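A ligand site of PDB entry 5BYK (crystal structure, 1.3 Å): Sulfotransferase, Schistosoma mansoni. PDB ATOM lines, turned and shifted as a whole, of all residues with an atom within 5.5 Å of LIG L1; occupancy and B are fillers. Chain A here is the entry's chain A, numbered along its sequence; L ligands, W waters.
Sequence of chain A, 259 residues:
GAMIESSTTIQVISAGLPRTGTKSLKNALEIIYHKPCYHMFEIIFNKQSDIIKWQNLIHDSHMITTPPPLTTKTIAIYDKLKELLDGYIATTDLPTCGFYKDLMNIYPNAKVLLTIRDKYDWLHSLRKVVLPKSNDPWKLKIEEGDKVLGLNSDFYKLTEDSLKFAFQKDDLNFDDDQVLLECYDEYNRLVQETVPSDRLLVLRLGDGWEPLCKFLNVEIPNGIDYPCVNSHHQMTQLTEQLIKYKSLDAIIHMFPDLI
Residues that only touch LIG L1: Ser 231 (3.4 Å), Val 229 (3.4 Å), Leu 205 (3.6 Å), CAS 228 (3.6 Å), Pro 18 (3.9 Å) and Tyr 226 (3.9 Å). Hydrophobic or aromatic side chains within 4 Å of LIG L1: Leu 205, Tyr 226 and His 232. Of the 23 residues printed, 17 come within 4 Å of LIG L1. The nearest printed residue that does not touch LIG L1 is Gly 206 (4.1 Å).
OG of Ser 125 is in hydrogen-bond range of NE of Arg 19. OG1 of Thr 22 sits at hydrogen-bond distance from NE2 of His 39. O of Pro 227 sits at hydrogen-bond distance from OG of Ser 24 (3.2 Å). N of Val 229 is in hydrogen-bond range of OG of Ser 24, 3.1 Å away. A ring nitrogen (NE2) of His 39 is in hydrogen-bond range of the backbone NH (N) of Lys 23 (3.4 Å). O of Arg 19 is in hydrogen-bond range of NH1 of Arg 117 (2.9 Å). NH2 of Arg 19 lies within hydrogen-bond range of O of Asn 230 (2.8 Å). OG1 of Thr 20 sits at hydrogen-bond distance from O of Leu 17 (2.6 Å).
OG of Ser 125 sits at hydrogen-bond distance from O2 of LIG L1. N of Thr 22 lies within hydrogen-bond range of O4 of LIG L1, 2.7 Å away. OG1 of Thr 22 is in hydrogen-bond range of O4 of LIG L1, at 2.7 Å. N2 of LIG L1 sits at hydrogen-bond distance from OG of Ser 24, 2.8 Å away. The backbone NH (N) of Lys 23 sits at hydrogen-bond distance from an oxygen (O5) of LIG L1, at 2.9 Å. NH2 of Arg 117 is in salt-bridge range of O1 of LIG L1, 2.9 Å away. An oxygen (O4) of LIG L1 lies within hydrogen-bond range of the backbone NH (N) of Arg 19, 2.9 Å away. NH1 of Arg 19 is in salt-bridge range of O6 of LIG L1 (2.9 Å). ND2 of Asn 230 is in hydrogen-bond range of O5 of LIG L1 (2.9 Å). O of Pro 227 sits at hydrogen-bond distance from N3 of LIG L1, 2.9 Å away. An oxygen (O7) of LIG L1 is in hydrogen-bond range of the backbone NH (N) of Gly 21, at 2.9 Å. O2 of LIG L1 is in hydrogen-bond range of N of His 232, at 2.9 Å. N of Thr 20 is in hydrogen-bond range of O4 of LIG L1.
Water W6 lies within hydrogen-bond range of O6 of LIG L1 (2.6 Å), O3 of LG2 L2 (2.8 Å), ND2 of Asn 230 (3.0 Å) and NH1 of Arg 19 (3.1 Å). Water W3 lies within hydrogen-bond range of O1 of LIG L1 (2.7 Å) and O of Asp 121 (2.8 Å). Water W1 lies within hydrogen-bond range of an oxygen (O5) of LIG L1 (2.7 Å), the backbone NH of Ser 24 (2.9 Å), the backbone carbonyl oxygen of Val 229 (3.0 Å) and the backbone NH of Lys 23 (3.3 Å). Water W2 bridges the backbone carbonyl oxygen of Tyr 226 and a nitrogen (N3) of LIG L1.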
ATOM      1  N   LEU A  17      -4.920  -0.963 -12.314  1.00  0.00           N
ATOM      2  CA  LEU A  17      -3.545  -0.497 -12.404  1.00  0.00           C
ATOM      3  C   LEU A  17      -3.438   0.974 -11.980  1.00  0.00           C
ATOM      4  O   LEU A  17      -4.423   1.701 -11.957  1.00  0.00           O
ATOM      5  CB  LEU A  17      -3.060  -0.670 -13.843  1.00  0.00           C
ATOM      6  CG  LEU A  17      -2.896  -2.126 -14.286  1.00  0.00           C
ATOM      7  CD1 LEU A  17      -2.805  -2.242 -15.798  1.00  0.00           C
ATOM      8  CD2 LEU A  17      -1.690  -2.768 -13.606  1.00  0.00           C
ATOM      9  N   PRO A  18      -2.220   1.437 -11.649  1.00  0.00           N
ATOM     10  CA  PRO A  18      -2.079   2.861 -11.369  1.00  0.00           C
ATOM     11  C   PRO A  18      -2.575   3.735 -12.532  1.00  0.00           C
ATOM     12  O   PRO A  18      -2.524   3.309 -13.696  1.00  0.00           O
ATOM     13  CB  PRO A  18      -0.561   3.048 -11.164  1.00  0.00           C
ATOM     14  CG  PRO A  18       0.066   1.780 -11.589  1.00  0.00           C
ATOM     15  CD  PRO A  18      -0.946   0.707 -11.502  1.00  0.00           C
ATOM     16  N   ARG A  19      -3.059   4.934 -12.196  1.00  0.00           N
ATOM     17  CA  ARG A  19      -3.580   5.917 -13.144  1.00  0.00           C
ATOM     18  C   ARG A  19      -4.929   5.521 -13.733  1.00  0.00           C
ATOM     19  O   ARG A  19      -5.261   5.945 -14.837  1.00  0.00           O
ATOM     20  CB  ARG A  19      -2.567   6.309 -14.242  1.00  0.00           C
ATOM     21  CG  ARG A  19      -1.144   6.624 -13.744  1.00  0.00           C
ATOM     22  CD  ARG A  19      -1.118   7.593 -12.556  1.00  0.00           C
ATOM     23  NE  ARG A  19      -1.625   8.902 -12.933  1.00  0.00           N
ATOM     24  CZ  ARG A  19      -1.836   9.899 -12.070  1.00  0.00           C
ATOM     25  NH1 ARG A  19      -1.602   9.729 -10.768  1.00  0.00           N
ATOM     26  NH2 ARG A  19      -2.278  11.086 -12.499  1.00  0.00           N
ATOM     27  N   THR A  20      -5.715   4.766 -12.972  1.00  0.00           N
ATOM     28  CA  THR A  20      -7.062   4.406 -13.384  1.00  0.00           C
ATOM     29  C   THR A  20      -8.125   4.833 -12.371  1.00  0.00           C
ATOM     30  O   THR A  20      -9.223   4.308 -12.366  1.00  0.00           O
ATOM     31  CB  THR A  20      -7.224   2.884 -13.629  1.00  0.00           C
ATOM     32  OG1 THR A  20      -6.970   2.170 -12.415  1.00  0.00           O
ATOM     33  CG2 THR A  20      -6.277   2.402 -14.724  1.00  0.00           C
ATOM     34  N   GLY A  21      -7.795   5.810 -11.526  1.00  0.00           N
ATOM     35  CA  GLY A  21      -8.715   6.270 -10.489  1.00  0.00           C
ATOM     36  C   GLY A  21      -8.546   5.567  -9.161  1.00  0.00           C
ATOM     37  O   GLY A  21      -9.475   5.556  -8.345  1.00  0.00           O
ATOM     38  N   THR A  22      -7.371   4.986  -8.911  1.00  0.00           N
ATOM     39  CA  THR A  22      -7.136   4.243  -7.673  1.00  0.00           C
ATOM     40  C   THR A  22      -7.135   5.131  -6.412  1.00  0.00           C
ATOM     41  O   THR A  22      -7.605   4.706  -5.347  1.00  0.00           O
ATOM     42  CB  THR A  22      -5.837   3.401  -7.723  1.00  0.00           C
ATOM     43  OG1 THR A  22      -4.715   4.275  -7.792  1.00  0.00           O
ATOM     44  CG2 THR A  22      -5.849   2.435  -8.910  1.00  0.00           C
ATOM     45  N   LYS A  23      -6.605   6.352  -6.508  1.00  0.00           N
ATOM     46  CA  LYS A  23      -6.557   7.179  -5.305  1.00  0.00           C
ATOM     47  C   LYS A  23      -7.962   7.685  -4.965  1.00  0.00           C
ATOM     48  O   LYS A  23      -8.348   7.746  -3.793  1.00  0.00           O
ATOM     49  CB  LYS A  23      -5.549   8.335  -5.458  1.00  0.00           C
ATOM     50  CG  LYS A  23      -5.381   9.206  -4.205  1.00  0.00           C
ATOM     51  CD  LYS A  23      -5.100   8.407  -2.960  1.00  0.00           C
ATOM     52  CE  LYS A  23      -4.572   9.242  -1.800  1.00  0.00           C
ATOM     53  NZ  LYS A  23      -5.552  10.094  -1.055  1.00  0.00           N
ATOM     54  N   SER A  24      -8.756   8.026  -5.992  1.00  0.00           N
ATOM     55  CA  SER A  24     -10.152   8.410  -5.757  1.00  0.00           C
ATOM     56  C   SER A  24     -10.902   7.242  -5.124  1.00  0.00           C
ATOM     57  O   SER A  24     -11.703   7.440  -4.204  1.00  0.00           O
ATOM     58  CB  SER A  24     -10.832   8.856  -7.046  1.00  0.00           C
ATOM     59  OG  SER A  24     -10.302  10.096  -7.455  1.00  0.00           O
ATOM     60  N   HIS A  39      -2.739   1.728  -0.668  1.00  0.00           N
ATOM     61  CA  HIS A  39      -2.492   2.412  -1.926  1.00  0.00           C
ATOM     62  C   HIS A  39      -1.000   2.722  -1.957  1.00  0.00           C
ATOM     63  O   HIS A  39      -0.365   2.698  -0.902  1.00  0.00           O
ATOM     64  CB  HIS A  39      -3.269   3.730  -1.957  1.00  0.00           C
ATOM     65  CG  HIS A  39      -3.258   4.426  -3.285  1.00  0.00           C
ATOM     66  ND1 HIS A  39      -2.291   5.349  -3.628  1.00  0.00           N
ATOM     67  CD2 HIS A  39      -4.105   4.346  -4.336  1.00  0.00           C
ATOM     68  CE1 HIS A  39      -2.526   5.774  -4.854  1.00  0.00           C
ATOM     69  NE2 HIS A  39      -3.639   5.214  -5.296  1.00  0.00           N
ATOM     70  N   ARG A 117      -9.828   2.522 -17.939  1.00  0.00           N
ATOM     71  CA  ARG A 117     -10.049   3.741 -18.708  1.00  0.00           C
ATOM     72  C   ARG A 117      -9.441   3.549 -20.091  1.00  0.00           C
ATOM     73  O   ARG A 117      -8.796   2.539 -20.368  1.00  0.00           O
ATOM     74  CB  ARG A 117      -9.378   4.950 -18.037  1.00  0.00           C
ATOM     75  CG  ARG A 117      -7.867   4.881 -18.090  1.00  0.00           C
ATOM     76  CD  ARG A 117      -7.189   5.968 -17.271  1.00  0.00           C
ATOM     77  NE  ARG A 117      -7.478   7.326 -17.739  1.00  0.00           N
ATOM     78  CZ  ARG A 117      -6.882   8.418 -17.277  1.00  0.00           C
ATOM     79  NH1 ARG A 117      -5.922   8.320 -16.370  1.00  0.00           N
ATOM     80  NH2 ARG A 117      -7.218   9.622 -17.732  1.00  0.00           N
ATOM     81  N   ASP A 121      -5.153   7.426 -22.753  1.00  0.00           N
ATOM     82  CA  ASP A 121      -5.217   8.338 -21.611  1.00  0.00           C
ATOM     83  C   ASP A 121      -4.420   7.768 -20.433  1.00  0.00           C
ATOM     84  O   ASP A 121      -3.723   8.501 -19.732  1.00  0.00           O
ATOM     85  CB  ASP A 121      -6.660   8.568 -21.152  1.00  0.00           C
ATOM     86  CG  ASP A 121      -7.488   9.373 -22.129  1.00  0.00           C
ATOM     87  OD1 ASP A 121      -6.956  10.046 -23.042  1.00  0.00           O
ATOM     88  OD2 ASP A 121      -8.727   9.329 -21.943  1.00  0.00           O
ATOM     89  N   SER A 125      -1.053   9.482 -18.812  1.00  0.00           N
ATOM     90  CA  SER A 125      -1.037   9.749 -17.384  1.00  0.00           C
ATOM     91  C   SER A 125       0.137   9.032 -16.694  1.00  0.00           C
ATOM     92  O   SER A 125       0.859   9.627 -15.883  1.00  0.00           O
ATOM     93  CB  SER A 125      -2.370   9.265 -16.791  1.00  0.00           C
ATOM     94  OG  SER A 125      -2.519   9.641 -15.443  1.00  0.00           O
ATOM     95  N   VAL A 129       3.548  10.756 -14.514  1.00  0.00           N
ATOM     96  CA  VAL A 129       3.550  10.617 -13.060  1.00  0.00           C
ATOM     97  C   VAL A 129       4.408   9.458 -12.565  1.00  0.00           C
ATOM     98  O   VAL A 129       5.225   9.622 -11.657  1.00  0.00           O
ATOM     99  CB  VAL A 129       2.110  10.452 -12.515  1.00  0.00           C
ATOM    100  CG1 VAL A 129       2.155  10.253 -10.996  1.00  0.00           C
ATOM    101  CG2 VAL A 129       1.250  11.646 -12.904  1.00  0.00           C
ATOM    102  N   LEU A 205     -13.642   5.197 -15.198  1.00  0.00           N
ATOM    103  CA  LEU A 205     -13.529   6.559 -14.653  1.00  0.00           C
ATOM    104  C   LEU A 205     -14.800   7.344 -14.937  1.00  0.00           C
ATOM    105  O   LEU A 205     -15.270   7.391 -16.081  1.00  0.00           O
ATOM    106  CB  LEU A 205     -12.370   7.322 -15.283  1.00  0.00           C
ATOM    107  CG  LEU A 205     -10.966   7.085 -14.745  1.00  0.00           C
ATOM    108  CD1 LEU A 205      -9.989   7.978 -15.493  1.00  0.00           C
ATOM    109  CD2 LEU A 205     -10.914   7.329 -13.232  1.00  0.00           C
ATOM    110  N   GLY A 206     -15.376   7.940 -13.896  1.00  0.00           N
ATOM    111  CA  GLY A 206     -16.598   8.704 -14.037  1.00  0.00           C
ATOM    112  C   GLY A 206     -17.837   7.974 -13.554  1.00  0.00           C
ATOM    113  O   GLY A 206     -18.904   8.571 -13.449  1.00  0.00           O
ATOM    114  N   TYR A 226     -18.424  11.957  -5.222  1.00  0.00           N
ATOM    115  CA  TYR A 226     -17.420  10.925  -5.425  1.00  0.00           C
ATOM    116  C   TYR A 226     -16.069  11.616  -5.639  1.00  0.00           C
ATOM    117  O   TYR A 226     -15.995  12.601  -6.379  1.00  0.00           O
ATOM    118  CB  TYR A 226     -17.775  10.046  -6.621  1.00  0.00           C
ATOM    119  CG  TYR A 226     -16.849   8.861  -6.747  1.00  0.00           C
ATOM    120  CD1 TYR A 226     -17.099   7.692  -6.059  1.00  0.00           C
ATOM    121  CD2 TYR A 226     -15.708   8.933  -7.539  1.00  0.00           C
ATOM    122  CE1 TYR A 226     -16.247   6.608  -6.155  1.00  0.00           C
ATOM    123  CE2 TYR A 226     -14.844   7.860  -7.645  1.00  0.00           C
ATOM    124  CZ  TYR A 226     -15.123   6.693  -6.951  1.00  0.00           C
ATOM    125  OH  TYR A 226     -14.265   5.615  -7.052  1.00  0.00           O
ATOM    126  N   PRO A 227     -15.005  11.105  -5.000  1.00  0.00           N
ATOM    127  CA  PRO A 227     -13.704  11.767  -5.084  1.00  0.00           C
ATOM    128  C   PRO A 227     -13.166  11.925  -6.509  1.00  0.00           C
ATOM    129  O   PRO A 227     -13.331  11.038  -7.354  1.00  0.00           O
ATOM    130  CB  PRO A 227     -12.783  10.825  -4.309  1.00  0.00           C
ATOM    131  CG  PRO A 227     -13.694  10.176  -3.322  1.00  0.00           C
ATOM    132  CD  PRO A 227     -14.984   9.974  -4.046  1.00  0.00           C
ATOM    133  N   CAS A 228     -12.516  13.061  -6.767  1.00  0.00           N
ATOM    134  CA  CAS A 228     -11.798  13.270  -8.011  1.00  0.00           C
ATOM    135  CB  CAS A 228     -12.537  14.227  -8.948  1.00  0.00           C
ATOM    136  C   CAS A 228     -10.482  13.870  -7.625  1.00  0.00           C
ATOM    137  O   CAS A 228     -10.372  15.108  -7.438  1.00  0.00           O
ATOM    138  SG  CAS A 228     -11.731  14.271 -10.521  1.00  0.00           S
ATOM    139 AS   CAS A 228     -10.391  16.092 -10.509  1.00  0.00          AS
ATOM    140  CE1 CAS A 228      -8.526  15.654  -9.971  1.00  0.00           C
ATOM    141  CE2 CAS A 228     -10.356  16.756 -12.377  1.00  0.00           C
ATOM    142  N   VAL A 229      -9.458  13.039  -7.456  1.00  0.00           N
ATOM    143  CA  VAL A 229      -8.157  13.504  -7.013  1.00  0.00           C
ATOM    144  C   VAL A 229      -7.072  12.810  -7.835  1.00  0.00           C
ATOM    145  O   VAL A 229      -7.340  11.817  -8.512  1.00  0.00           O
ATOM    146  CB  VAL A 229      -7.916  13.202  -5.512  1.00  0.00           C
ATOM    147  CG1 VAL A 229      -8.905  13.946  -4.622  1.00  0.00           C
ATOM    148  CG2 VAL A 229      -7.984  11.706  -5.259  1.00  0.00           C
ATOM    149  N   ASN A 230      -5.857  13.357  -7.782  1.00  0.00           N
ATOM    150  CA  ASN A 230      -4.667  12.708  -8.319  1.00  0.00           C
ATOM    151  C   ASN A 230      -4.562  12.819  -9.836  1.00  0.00           C
ATOM    152  O   ASN A 230      -4.076  11.903 -10.502  1.00  0.00           O
ATOM    153  CB  ASN A 230      -4.555  11.247  -7.842  1.00  0.00           C
ATOM    154  CG  ASN A 230      -3.137  10.694  -7.908  1.00  0.00           C
ATOM    155  OD1 ASN A 230      -2.161  11.424  -8.063  1.00  0.00           O
ATOM    156  ND2 ASN A 230      -3.029   9.376  -7.780  1.00  0.00           N
ATOM    157  N   SER A 231      -5.009  13.934 -10.408  1.00  0.00           N
ATOM    158  CA  SER A 231      -4.787  14.190 -11.833  1.00  0.00           C
ATOM    159  C   SER A 231      -3.293  14.398 -12.059  1.00  0.00           C
ATOM    160  O   SER A 231      -2.553  14.812 -11.140  1.00  0.00           O
ATOM    161  CB  SER A 231      -5.544  15.428 -12.302  1.00  0.00           C
ATOM    162  OG  SER A 231      -5.007  16.597 -11.715  1.00  0.00           O
ATOM    163  N   HIS A 232      -2.830  14.139 -13.279  1.00  0.00           N
ATOM    164  CA  HIS A 232      -1.412  14.375 -13.546  1.00  0.00           C
ATOM    165  C   HIS A 232      -1.068  15.845 -13.357  1.00  0.00           C
ATOM    166  O   HIS A 232       0.041  16.171 -12.928  1.00  0.00           O
ATOM    167  CB  HIS A 232      -0.949  13.834 -14.900  1.00  0.00           C
ATOM    168  CG  HIS A 232      -1.489  14.548 -16.098  1.00  0.00           C
ATOM    169  ND1 HIS A 232      -1.030  15.784 -16.502  1.00  0.00           N
ATOM    170  CD2 HIS A 232      -2.432  14.187 -17.008  1.00  0.00           C
ATOM    171  CE1 HIS A 232      -1.677  16.157 -17.587  1.00  0.00           C
ATOM    172  NE2 HIS A 232      -2.530  15.207 -17.912  1.00  0.00           N
ATOM    173  N   HIS A 233      -2.011  16.739 -13.654  1.00  0.00           N
ATOM    174  CA  HIS A 233      -1.769  18.167 -13.443  1.00  0.00           C
ATOM    175  C   HIS A 233      -1.494  18.464 -11.967  1.00  0.00           C
ATOM    176  O   HIS A 233      -0.590  19.229 -11.623  1.00  0.00           O
ATOM    177  CB  HIS A 233      -2.951  19.023 -13.919  1.00  0.00           C
ATOM    178  CG  HIS A 233      -3.141  19.040 -15.402  1.00  0.00           C
ATOM    179  ND1 HIS A 233      -2.168  19.505 -16.269  1.00  0.00           N
ATOM    180  CD2 HIS A 233      -4.187  18.669 -16.167  1.00  0.00           C
ATOM    181  CE1 HIS A 233      -2.620  19.408 -17.510  1.00  0.00           C
ATOM    182  NE2 HIS A 233      -3.836  18.899 -17.474  1.00  0.00           N
HETATM  183  P1  LIG L   1      -5.174  11.961 -15.380  1.00  0.00           P
HETATM  184  O1  LIG L   1      -5.360  11.594 -16.828  1.00  0.00           O
HETATM  185  O2  LIG L   1      -3.736  11.880 -14.931  1.00  0.00           O
HETATM  186  O3  LIG L   1      -5.752  13.282 -14.969  1.00  0.00           O
HETATM  187  P2  LIG L   1      -4.695   7.050  -9.947  1.00  0.00           P
HETATM  188  O4  LIG L   1      -4.973   5.565 -10.109  1.00  0.00           O
HETATM  189  O5  LIG L   1      -5.189   7.620  -8.641  1.00  0.00           O
HETATM  190  O6  LIG L   1      -3.215   7.345 -10.203  1.00  0.00           O
HETATM  191  O7  LIG L   1      -5.582   7.684 -11.119  1.00  0.00           O
HETATM  192  C1  LIG L   1      -5.519   9.090 -11.412  1.00  0.00           C
HETATM  193  C2  LIG L   1      -6.212   9.353 -12.723  1.00  0.00           C
HETATM  194  O8  LIG L   1      -7.652   9.140 -12.580  1.00  0.00           O
HETATM  195  C3  LIG L   1      -6.055  10.780 -13.159  1.00  0.00           C
HETATM  196  O9  LIG L   1      -5.998  10.818 -14.601  1.00  0.00           O
HETATM  197  C4  LIG L   1      -7.267  11.424 -12.593  1.00  0.00           C
HETATM  198  O10 LIG L   1      -7.600  12.674 -13.175  1.00  0.00           O
HETATM  199  C5  LIG L   1      -8.315  10.376 -12.861  1.00  0.00           C
HETATM  200  N1  LIG L   1      -9.454  10.463 -12.010  1.00  0.00           N
HETATM  201  C6  LIG L   1      -9.476  10.233 -10.685  1.00  0.00           C
HETATM  202  N2  LIG L   1     -10.707  10.383 -10.193  1.00  0.00           N
HETATM  203  C7  LIG L   1     -11.520  10.712 -11.239  1.00  0.00           C
HETATM  204  C8  LIG L   1     -12.904  11.013 -11.372  1.00  0.00           C
HETATM  205  N3  LIG L   1     -13.733  10.985 -10.253  1.00  0.00           N
HETATM  206  N4  LIG L   1     -13.392  11.318 -12.586  1.00  0.00           N
HETATM  207  C9  LIG L   1     -12.593  11.339 -13.647  1.00  0.00           C
HETATM  208  N5  LIG L   1     -11.299  11.077 -13.584  1.00  0.00           N
HETATM  209  C10 LIG L   1     -10.724  10.775 -12.398  1.00  0.00           C
HETATM  210  C1  LG2 L   2       2.264   6.718  -7.536  1.00  0.00           C
HETATM  211  C2  LG2 L   2       2.370   5.394  -7.950  1.00  0.00           C
HETATM  212  C3  LG2 L   2       3.628   4.909  -8.309  1.00  0.00           C
HETATM  213  C4  LG2 L   2       4.750   5.721  -8.249  1.00  0.00           C
HETATM  214  C5  LG2 L   2       4.630   7.043  -7.836  1.00  0.00           C
HETATM  215  C6  LG2 L   2       3.383   7.547  -7.479  1.00  0.00           C
HETATM  216  C7  LG2 L   2       5.600   9.328  -7.782  1.00  0.00           C
HETATM  217  C8  LG2 L   2       4.140   9.705  -7.959  1.00  0.00           C
HETATM  218  C9  LG2 L   2       3.257   8.866  -7.078  1.00  0.00           C
HETATM  219  C10 LG2 L   2       1.226   4.588  -7.991  1.00  0.00           C
HETATM  220  C11 LG2 L   2       6.205  10.031  -6.564  1.00  0.00           C
HETATM  221  C12 LG2 L   2       5.206  12.639  -5.596  1.00  0.00           C
HETATM  222  C13 LG2 L   2       7.285  13.675  -6.523  1.00  0.00           C
HETATM  223  C14 LG2 L   2       6.652  12.384  -6.000  1.00  0.00           C
HETATM  224  N1  LG2 L   2       5.780   7.856  -7.800  1.00  0.00           N
HETATM  225  N2  LG2 L   2       3.777   3.626  -8.697  1.00  0.00           N
HETATM  226  N3  LG2 L   2       6.740  11.341  -7.025  1.00  0.00           N
HETATM  227  O1  LG2 L   2       4.816   2.998  -8.245  1.00  0.00           O
HETATM  228  O2  LG2 L   2       2.855   2.965  -9.651  1.00  0.00           O
HETATM  229  O3  LG2 L   2       0.083   5.249  -7.458  1.00  0.00           O
HETATM  230  O   HOH W   1      -7.590   8.871  -8.479  1.00  0.00           O
HETATM  231  O   HOH W   2     -16.431  12.551  -9.149  1.00  0.00           O
HETATM  232  O   HOH W   3      -4.261  11.247 -19.258  1.00  0.00           O
HETATM  233  O   HOH W   4     -17.026  10.404 -10.556  1.00  0.00           O
HETATM  234  O   HOH W   5     -10.321  11.921 -16.219  1.00  0.00           O
HETATM  235  O   HOH W   6      -1.000   7.402  -8.786  1.00  0.00           O
HETATM  236  O   HOH W   7     -15.903  12.534 -13.212  1.00  0.00           O
